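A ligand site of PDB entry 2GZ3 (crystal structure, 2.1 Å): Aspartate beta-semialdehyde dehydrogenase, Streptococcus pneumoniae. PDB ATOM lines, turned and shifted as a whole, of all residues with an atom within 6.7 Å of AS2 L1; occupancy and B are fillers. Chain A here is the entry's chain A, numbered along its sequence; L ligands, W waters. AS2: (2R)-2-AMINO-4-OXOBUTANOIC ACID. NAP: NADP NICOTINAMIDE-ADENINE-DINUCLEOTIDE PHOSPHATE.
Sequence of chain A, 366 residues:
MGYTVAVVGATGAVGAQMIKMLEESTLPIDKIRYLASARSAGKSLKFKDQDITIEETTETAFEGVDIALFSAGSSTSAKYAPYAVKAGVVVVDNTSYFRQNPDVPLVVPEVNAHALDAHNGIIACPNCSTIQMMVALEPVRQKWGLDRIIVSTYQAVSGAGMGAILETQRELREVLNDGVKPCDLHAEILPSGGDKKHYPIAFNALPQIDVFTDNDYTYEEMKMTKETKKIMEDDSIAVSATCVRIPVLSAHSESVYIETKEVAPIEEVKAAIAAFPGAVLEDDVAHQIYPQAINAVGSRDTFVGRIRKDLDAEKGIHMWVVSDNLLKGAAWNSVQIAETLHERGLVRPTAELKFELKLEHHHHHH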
ATOM      1  N   ASN A  94      25.017  17.541   4.291  1.00  0.00           N
ATOM      2  CA  ASN A  94      24.240  16.683   3.394  1.00  0.00           C
ATOM      3  C   ASN A  94      24.533  16.866   1.912  1.00  0.00           C
ATOM      4  O   ASN A  94      24.209  15.996   1.099  1.00  0.00           O
ATOM      5  CB  ASN A  94      22.742  16.845   3.622  1.00  0.00           C
ATOM      6  CG  ASN A  94      22.210  15.895   4.662  1.00  0.00           C
ATOM      7  OD1 ASN A  94      21.750  16.320   5.727  1.00  0.00           O
ATOM      8  ND2 ASN A  94      22.265  14.590   4.360  1.00  0.00           N
ATOM      9  N   ARG A  99      32.073  16.371  -0.547  1.00  0.00           N
ATOM     10  CA  ARG A  99      32.177  14.906  -0.590  1.00  0.00           C
ATOM     11  C   ARG A  99      33.464  14.351  -1.192  1.00  0.00           C
ATOM     12  O   ARG A  99      33.939  13.271  -0.789  1.00  0.00           O
ATOM     13  CB  ARG A  99      30.993  14.304  -1.358  1.00  0.00           C
ATOM     14  CG  ARG A  99      29.655  14.434  -0.645  1.00  0.00           C
ATOM     15  CD  ARG A  99      28.552  13.875  -1.506  1.00  0.00           C
ATOM     16  NE  ARG A  99      27.231  14.208  -1.012  1.00  0.00           N
ATOM     17  CZ  ARG A  99      26.128  14.230  -1.775  1.00  0.00           C
ATOM     18  NH1 ARG A  99      26.222  13.936  -3.073  1.00  0.00           N
ATOM     19  NH2 ARG A  99      24.941  14.538  -1.244  1.00  0.00           N
ATOM     20  N   PRO A 126      26.786  11.065   1.983  1.00  0.00           N
ATOM     21  CA  PRO A 126      26.747  10.841   0.537  1.00  0.00           C
ATOM     22  C   PRO A 126      25.385  11.099  -0.084  1.00  0.00           C
ATOM     23  O   PRO A 126      24.378  11.291   0.605  1.00  0.00           O
ATOM     24  CB  PRO A 126      27.101   9.341   0.374  1.00  0.00           C
ATOM     25  CG  PRO A 126      27.559   8.895   1.697  1.00  0.00           C
ATOM     26  CD  PRO A 126      27.017   9.810   2.726  1.00  0.00           C
ATOM     27  N   ASN A 127      25.396  11.087  -1.408  1.00  0.00           N
ATOM     28  CA  ASN A 127      24.226  11.140  -2.228  1.00  0.00           C
ATOM     29  C   ASN A 127      23.239  10.052  -1.794  1.00  0.00           C
ATOM     30  O   ASN A 127      23.657   8.928  -1.475  1.00  0.00           O
ATOM     31  CB  ASN A 127      24.695  10.964  -3.685  1.00  0.00           C
ATOM     32  CG  ASN A 127      23.595  10.552  -4.599  1.00  0.00           C
ATOM     33  OD1 ASN A 127      23.550   9.404  -5.046  1.00  0.00           O
ATOM     34  ND2 ASN A 127      22.704  11.487  -4.899  1.00  0.00           N
ATOM     35  N   CYS A 128      21.943  10.383  -1.766  1.00  0.00           N
ATOM     36  CA  CYS A 128      20.906   9.468  -1.258  1.00  0.00           C
ATOM     37  C   CYS A 128      20.779   8.143  -2.013  1.00  0.00           C
ATOM     38  O   CYS A 128      20.650   7.081  -1.399  1.00  0.00           O
ATOM     39  CB  CYS A 128      19.562  10.190  -1.155  1.00  0.00           C
ATOM     40  SG  CYS A 128      19.037  10.966  -2.629  1.00  0.00           S
ATOM     41  N   SER A 129      20.832   8.213  -3.349  1.00  0.00           N
ATOM     42  CA  SER A 129      20.877   7.047  -4.232  1.00  0.00           C
ATOM     43  C   SER A 129      22.046   6.135  -3.913  1.00  0.00           C
ATOM     44  O   SER A 129      21.923   4.916  -3.878  1.00  0.00           O
ATOM     45  CB  SER A 129      20.985   7.495  -5.698  1.00  0.00           C
ATOM     46  OG  SER A 129      20.292   8.704  -5.904  1.00  0.00           O
ATOM     47  N   ILE A 131      23.870   6.049  -0.951  1.00  0.00           N
ATOM     48  CA  ILE A 131      23.722   5.484   0.394  1.00  0.00           C
ATOM     49  C   ILE A 131      23.004   4.140   0.339  1.00  0.00           C
ATOM     50  O   ILE A 131      23.533   3.113   0.786  1.00  0.00           O
ATOM     51  CB  ILE A 131      23.014   6.487   1.362  1.00  0.00           C
ATOM     52  CG1 ILE A 131      23.913   7.711   1.648  1.00  0.00           C
ATOM     53  CG2 ILE A 131      22.620   5.785   2.671  1.00  0.00           C
ATOM     54  CD1 ILE A 131      23.196   8.909   2.267  1.00  0.00           C
ATOM     55  N   GLN A 155      13.734   7.727  -9.147  1.00  0.00           N
ATOM     56  CA  GLN A 155      13.847   8.700  -8.058  1.00  0.00           C
ATOM     57  C   GLN A 155      12.609   9.565  -7.808  1.00  0.00           C
ATOM     58  O   GLN A 155      11.935  10.006  -8.743  1.00  0.00           O
ATOM     59  CB  GLN A 155      15.126   9.539  -8.200  1.00  0.00           C
ATOM     60  CG  GLN A 155      16.371   8.724  -7.839  1.00  0.00           C
ATOM     61  CD  GLN A 155      17.663   9.437  -8.110  1.00  0.00           C
ATOM     62  OE1 GLN A 155      18.490   8.952  -8.880  1.00  0.00           O
ATOM     63  NE2 GLN A 155      17.879  10.571  -7.456  1.00  0.00           N
ATOM     64  N   ALA A 156      12.331   9.766  -6.517  1.00  0.00           N
ATOM     65  CA  ALA A 156      11.199  10.535  -6.019  1.00  0.00           C
ATOM     66  C   ALA A 156      11.530  12.019  -6.008  1.00  0.00           C
ATOM     67  O   ALA A 156      12.706  12.412  -5.834  1.00  0.00           O
ATOM     68  CB  ALA A 156      10.836  10.064  -4.600  1.00  0.00           C
ATOM     69  N   VAL A 157      10.492  12.838  -6.171  1.00  0.00           N
ATOM     70  CA  VAL A 157      10.640  14.286  -6.339  1.00  0.00           C
ATOM     71  C   VAL A 157      11.085  15.012  -5.078  1.00  0.00           C
ATOM     72  O   VAL A 157      11.672  16.094  -5.169  1.00  0.00           O
ATOM     73  CB  VAL A 157       9.343  14.961  -6.918  1.00  0.00           C
ATOM     74  CG1 VAL A 157       8.896  14.277  -8.226  1.00  0.00           C
ATOM     75  CG2 VAL A 157       8.211  14.941  -5.912  1.00  0.00           C
ATOM     76  N   SER A 158      10.796  14.427  -3.902  1.00  0.00           N
ATOM     77  CA  SER A 158      11.269  14.975  -2.613  1.00  0.00           C
ATOM     78  C   SER A 158      12.778  15.135  -2.583  1.00  0.00           C
ATOM     79  O   SER A 158      13.294  16.014  -1.906  1.00  0.00           O
ATOM     80  CB  SER A 158      10.810  14.131  -1.422  1.00  0.00           C
ATOM     81  OG  SER A 158      11.524  12.907  -1.374  1.00  0.00           O
ATOM     82  N   GLY A 159      13.486  14.296  -3.346  1.00  0.00           N
ATOM     83  CA  GLY A 159      14.934  14.473  -3.549  1.00  0.00           C
ATOM     84  C   GLY A 159      15.350  15.852  -4.060  1.00  0.00           C
ATOM     85  O   GLY A 159      16.466  16.323  -3.812  1.00  0.00           O
ATOM     86  N   ALA A 160      14.468  16.517  -4.797  1.00  0.00           N
ATOM     87  CA  ALA A 160      14.759  17.832  -5.352  1.00  0.00           C
ATOM     88  C   ALA A 160      14.188  18.990  -4.521  1.00  0.00           C
ATOM     89  O   ALA A 160      14.218  20.137  -4.931  1.00  0.00           O
ATOM     90  CB  ALA A 160      14.275  17.897  -6.810  1.00  0.00           C
ATOM     91  N   ILE A 209      18.580  14.101 -13.836  1.00  0.00           N
ATOM     92  CA  ILE A 209      18.632  14.539 -12.468  1.00  0.00           C
ATOM     93  C   ILE A 209      19.948  15.276 -12.383  1.00  0.00           C
ATOM     94  O   ILE A 209      20.983  14.746 -12.770  1.00  0.00           O
ATOM     95  CB  ILE A 209      18.555  13.342 -11.455  1.00  0.00           C
ATOM     96  CG1 ILE A 209      17.203  12.625 -11.611  1.00  0.00           C
ATOM     97  CG2 ILE A 209      18.731  13.848 -10.011  1.00  0.00           C
ATOM     98  CD1 ILE A 209      16.891  11.581 -10.583  1.00  0.00           C
ATOM     99  N   ASP A 210      19.894  16.508 -11.880  1.00  0.00           N
ATOM    100  CA  ASP A 210      21.033  17.437 -11.920  1.00  0.00           C
ATOM    101  C   ASP A 210      21.353  17.806 -13.383  1.00  0.00           C
ATOM    102  O   ASP A 210      20.711  17.322 -14.320  1.00  0.00           O
ATOM    103  CB  ASP A 210      22.264  16.855 -11.200  1.00  0.00           C
ATOM    104  CG  ASP A 210      22.944  17.880 -10.288  1.00  0.00           C
ATOM    105  OD1 ASP A 210      23.185  19.039 -10.733  1.00  0.00           O
ATOM    106  OD2 ASP A 210      23.238  17.532  -9.119  1.00  0.00           O
ATOM    107  N   GLU A 220      24.178  13.626 -11.126  1.00  0.00           N
ATOM    108  CA  GLU A 220      23.592  12.626 -10.236  1.00  0.00           C
ATOM    109  C   GLU A 220      24.212  11.266 -10.508  1.00  0.00           C
ATOM    110  O   GLU A 220      24.550  10.528  -9.572  1.00  0.00           O
ATOM    111  CB  GLU A 220      22.059  12.595 -10.356  1.00  0.00           C
ATOM    112  CG  GLU A 220      21.336  11.574  -9.477  1.00  0.00           C
ATOM    113  CD  GLU A 220      21.095  12.039  -8.031  1.00  0.00           C
ATOM    114  OE1 GLU A 220      21.502  13.173  -7.672  1.00  0.00           O
ATOM    115  OE2 GLU A 220      20.483  11.261  -7.236  1.00  0.00           O
ATOM    116  N   LYS A 223      27.924  11.191  -9.480  1.00  0.00           N
ATOM    117  CA  LYS A 223      28.011  11.080  -8.027  1.00  0.00           C
ATOM    118  C   LYS A 223      27.971   9.636  -7.595  1.00  0.00           C
ATOM    119  O   LYS A 223      28.772   9.189  -6.777  1.00  0.00           O
ATOM    120  CB  LYS A 223      26.855  11.823  -7.376  1.00  0.00           C
ATOM    121  CG  LYS A 223      26.924  13.315  -7.523  1.00  0.00           C
ATOM    122  CD  LYS A 223      25.559  13.900  -7.274  1.00  0.00           C
ATOM    123  CE  LYS A 223      25.601  15.397  -7.219  1.00  0.00           C
ATOM    124  NZ  LYS A 223      24.232  15.847  -6.873  1.00  0.00           N
ATOM    125  N   ARG A 245      13.870  10.658 -12.818  1.00  0.00           N
ATOM    126  CA  ARG A 245      12.861  11.144 -11.903  1.00  0.00           C
ATOM    127  C   ARG A 245      11.489  10.659 -12.346  1.00  0.00           C
ATOM    128  O   ARG A 245      11.165  10.773 -13.509  1.00  0.00           O
ATOM    129  CB  ARG A 245      12.885  12.688 -11.836  1.00  0.00           C
ATOM    130  CG  ARG A 245      12.122  13.275 -10.657  1.00  0.00           C
ATOM    131  CD  ARG A 245      12.929  13.132  -9.359  1.00  0.00           C
ATOM    132  NE  ARG A 245      14.079  14.023  -9.355  1.00  0.00           N
ATOM    133  CZ  ARG A 245      14.964  14.123  -8.364  1.00  0.00           C
ATOM    134  NH1 ARG A 245      14.835  13.396  -7.263  1.00  0.00           N
ATOM    135  NH2 ARG A 245      15.979  14.984  -8.481  1.00  0.00           N
ATOM    136  N   HIS A 252      13.332   6.523  -3.000  1.00  0.00           N
ATOM    137  CA  HIS A 252      13.991   6.161  -4.249  1.00  0.00           C
ATOM    138  C   HIS A 252      14.029   4.622  -4.389  1.00  0.00           C
ATOM    139  O   HIS A 252      14.224   3.922  -3.401  1.00  0.00           O
ATOM    140  CB  HIS A 252      15.406   6.732  -4.285  1.00  0.00           C
ATOM    141  CG  HIS A 252      15.476   8.237  -4.345  1.00  0.00           C
ATOM    142  ND1 HIS A 252      14.385   9.049  -4.513  1.00  0.00           N
ATOM    143  CD2 HIS A 252      16.550   9.071  -4.283  1.00  0.00           C
ATOM    144  CE1 HIS A 252      14.759  10.317  -4.528  1.00  0.00           C
ATOM    145  NE2 HIS A 252      16.074  10.362  -4.409  1.00  0.00           N
ATOM    146  N   ASN A 325      14.549   8.406   0.800  1.00  0.00           N
ATOM    147  CA  ASN A 325      15.616   9.336   0.443  1.00  0.00           C
ATOM    148  C   ASN A 325      15.790  10.475   1.431  1.00  0.00           C
ATOM    149  O   ASN A 325      16.842  11.111   1.482  1.00  0.00           O
ATOM    150  CB  ASN A 325      15.375   9.889  -0.967  1.00  0.00           C
ATOM    151  CG  ASN A 325      14.025  10.608  -1.107  1.00  0.00           C
ATOM    152  OD1 ASN A 325      12.949   9.984  -1.084  1.00  0.00           O
ATOM    153  ND2 ASN A 325      14.081  11.921  -1.298  1.00  0.00           N
ATOM    154  N   GLY A 329      18.540   8.141   3.217  1.00  0.00           N
ATOM    155  CA  GLY A 329      19.205   8.892   2.146  1.00  0.00           C
ATOM    156  C   GLY A 329      19.796  10.254   2.510  1.00  0.00           C
ATOM    157  O   GLY A 329      20.569  10.827   1.738  1.00  0.00           O
ATOM    158  N   ALA A 330      19.446  10.766   3.692  1.00  0.00           N
ATOM    159  CA  ALA A 330      19.814  12.123   4.096  1.00  0.00           C
ATOM    160  C   ALA A 330      19.799  12.293   5.605  1.00  0.00           C
ATOM    161  O   ALA A 330      20.814  12.094   6.252  1.00  0.00           O
ATOM    162  CB  ALA A 330      18.891  13.151   3.470  1.00  0.00           C
HETATM  163  O   AS2 L   1      17.991  14.387  -6.742  1.00  0.00           O
HETATM  164  C   AS2 L   1      17.916  13.705  -5.716  1.00  0.00           C
HETATM  165  OXT AS2 L   1      17.042  12.834  -5.636  1.00  0.00           O
HETATM  166  CA  AS2 L   1      18.903  14.010  -4.578  1.00  0.00           C
HETATM  167  N   AS2 L   1      20.284  13.714  -5.054  1.00  0.00           N
HETATM  168  CB  AS2 L   1      18.529  13.285  -3.291  1.00  0.00           C
HETATM  169  CG  AS2 L   1      19.654  12.455  -2.658  1.00  0.00           C
HETATM  170  OD2 AS2 L   1      20.706  12.974  -2.296  1.00  0.00           O
HETATM  171  PA  NAP L   2      14.374  22.442   0.249  1.00  0.00           P
HETATM  172  O1A NAP L   2      14.165  23.245  -0.996  1.00  0.00           O
HETATM  173  O2A NAP L   2      13.261  21.635   0.767  1.00  0.00           O
HETATM  174  O5B NAP L   2      14.830  23.465   1.382  1.00  0.00           O
HETATM  175  C5B NAP L   2      16.146  24.023   1.323  1.00  0.00           C
HETATM  176  C4B NAP L   2      16.572  24.572   2.671  1.00  0.00           C
HETATM  177  O4B NAP L   2      17.749  25.377   2.408  1.00  0.00           O
HETATM  178  C3B NAP L   2      15.556  25.512   3.337  1.00  0.00           C
HETATM  179  O3B NAP L   2      15.602  25.307   4.758  1.00  0.00           O
HETATM  180  C2B NAP L   2      16.116  26.910   3.005  1.00  0.00           C
HETATM  181  O2B NAP L   2      15.752  27.860   4.013  1.00  0.00           O
HETATM  182  C1B NAP L   2      17.608  26.603   3.119  1.00  0.00           C
HETATM  183  N9A NAP L   2      18.391  27.703   2.509  1.00  0.00           N
HETATM  184  C8A NAP L   2      18.341  28.115   1.238  1.00  0.00           C
HETATM  185  N7A NAP L   2      19.181  29.136   1.054  1.00  0.00           N
HETATM  186  C5A NAP L   2      19.791  29.369   2.229  1.00  0.00           C
HETATM  187  C6A NAP L   2      20.746  30.293   2.653  1.00  0.00           C
HETATM  188  N6A NAP L   2      21.259  31.182   1.791  1.00  0.00           N
HETATM  189  N1A NAP L   2      21.147  30.262   3.930  1.00  0.00           N
HETATM  190  C2A NAP L   2      20.645  29.366   4.788  1.00  0.00           C
HETATM  191  N3A NAP L   2      19.721  28.475   4.423  1.00  0.00           N
HETATM  192  C4A NAP L   2      19.279  28.457   3.151  1.00  0.00           C
HETATM  193  O3  NAP L   2      15.738  21.550   0.081  1.00  0.00           O
HETATM  194  PN  NAP L   2      16.096  19.986   0.577  1.00  0.00           P
HETATM  195  O1N NAP L   2      16.314  19.185  -0.669  1.00  0.00           O
HETATM  196  O2N NAP L   2      15.156  19.478   1.594  1.00  0.00           O
HETATM  197  O5D NAP L   2      17.547  20.260   1.302  1.00  0.00           O
HETATM  198  C5D NAP L   2      18.588  21.047   0.667  1.00  0.00           C
HETATM  199  C4D NAP L   2      19.959  20.312   0.648  1.00  0.00           C
HETATM  200  O4D NAP L   2      19.910  18.959   1.235  1.00  0.00           O
HETATM  201  C3D NAP L   2      20.434  20.158  -0.807  1.00  0.00           C
HETATM  202  O3D NAP L   2      21.811  20.499  -0.865  1.00  0.00           O
HETATM  203  C2D NAP L   2      20.256  18.660  -1.072  1.00  0.00           C
HETATM  204  O2D NAP L   2      21.175  18.152  -2.056  1.00  0.00           O
HETATM  205  C1D NAP L   2      20.597  18.082   0.292  1.00  0.00           C
HETATM  206  N1N NAP L   2      20.099  16.691   0.296  1.00  0.00           N
HETATM  207  C2N NAP L   2      18.812  16.436  -0.183  1.00  0.00           C
HETATM  208  C3N NAP L   2      18.319  15.142  -0.196  1.00  0.00           C
HETATM  209  C7N NAP L   2      16.917  14.875  -0.714  1.00  0.00           C
HETATM  210  O7N NAP L   2      16.451  13.715  -0.748  1.00  0.00           O
HETATM  211  N7N NAP L   2      16.268  15.975  -1.110  1.00  0.00           N
HETATM  212  C4N NAP L   2      19.118  14.108   0.256  1.00  0.00           C
HETATM  213  C5N NAP L   2      20.425  14.199   0.746  1.00  0.00           C
HETATM  214  C6N NAP L   2      21.003  15.616   0.783  1.00  0.00           C
HETATM  215  P2B NAP L   2      14.551  28.978   3.821  1.00  0.00           P
HETATM  216  O1X NAP L   2      15.015  30.234   4.690  1.00  0.00           O
HETATM  217  O2X NAP L   2      14.633  29.447   2.282  1.00  0.00           O
HETATM  218  O3X NAP L   2      13.273  28.359   4.252  1.00  0.00           O
HETATM  219  O   HOH W   1      23.395  14.787  -4.113  1.00  0.00           O
HETATM  220  O   HOH W   2      18.742  17.235  -6.916  1.00  0.00           O
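OE1 of Glu 220 is in salt-bridge range of N of AS2 L1, 2.9 Å away. NE2 of Gln 155 lies within hydrogen-bond range of OXT of AS2 L1 (3.0 Å). ND2 of Asn 325 sits at hydrogen-bond distance from O7N of NAP L2, at 3.0 Å. A carbon (CG) of AS2 L1 is bonded to the side-chain sulfur of Cys 128 (1.6 Å). ND2 of Asn 127 lies close to N of AS2 L1, at 3.3 Å. NH2 of Arg 245 is in salt-bridge range of O of AS2 L1, 2.7 Å away. O of Gly 159 is in hydrogen-bond range of N7N of NAP L2. N7N of NAP L2 sits at hydrogen-bond distance from O of Ser 158. N of Cys 128 is in hydrogen-bond range of OD2 of AS2 L1 (2.9 Å). NE2 of His 252 is in hydrogen-bond range of OXT of AS2 L1 (2.9 Å).
ND2 of Asn 127 is in hydrogen-bond range of OE2 of Glu 220, 3.2 Å away. O of Ala 156 is in hydrogen-bond range of NH1 of Arg 245 (2.7 Å). OE1 of Glu 220 is in salt-bridge range of NZ of Lys 223 (3.9 Å). NE2 of Gln 155 sits at hydrogen-bond distance from OE2 of Glu 220, at 2.7 Å. The side-chain amide oxygen (OD1) of Asn 127 lies close to the backbone NH (N) of Ser 129 (3.4 Å). OG of Ser 129 is in hydrogen-bond range of NE2 of Gln 155, 3.4 Å away. The side-chain sulfur of Cys 128 lies within hydrogen-bond range of a ring nitrogen (NE2) of His 252 (3.5 Å). A ring nitrogen (ND1) of His 252 sits at hydrogen-bond distance from the backbone NH of Ala 156, 3.0 Å away.
CA of Gly 159 touches OXT of AS2 L1 (3.4 Å). CG2 of Ile 209 touches O of AS2 L1, at 3.4 Å. Of the 22 residues printed, 8 come within 4 Å of AS2 L1. Along chain A the residues within 4 Å of AS2 L1 span positions 127 to 252.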
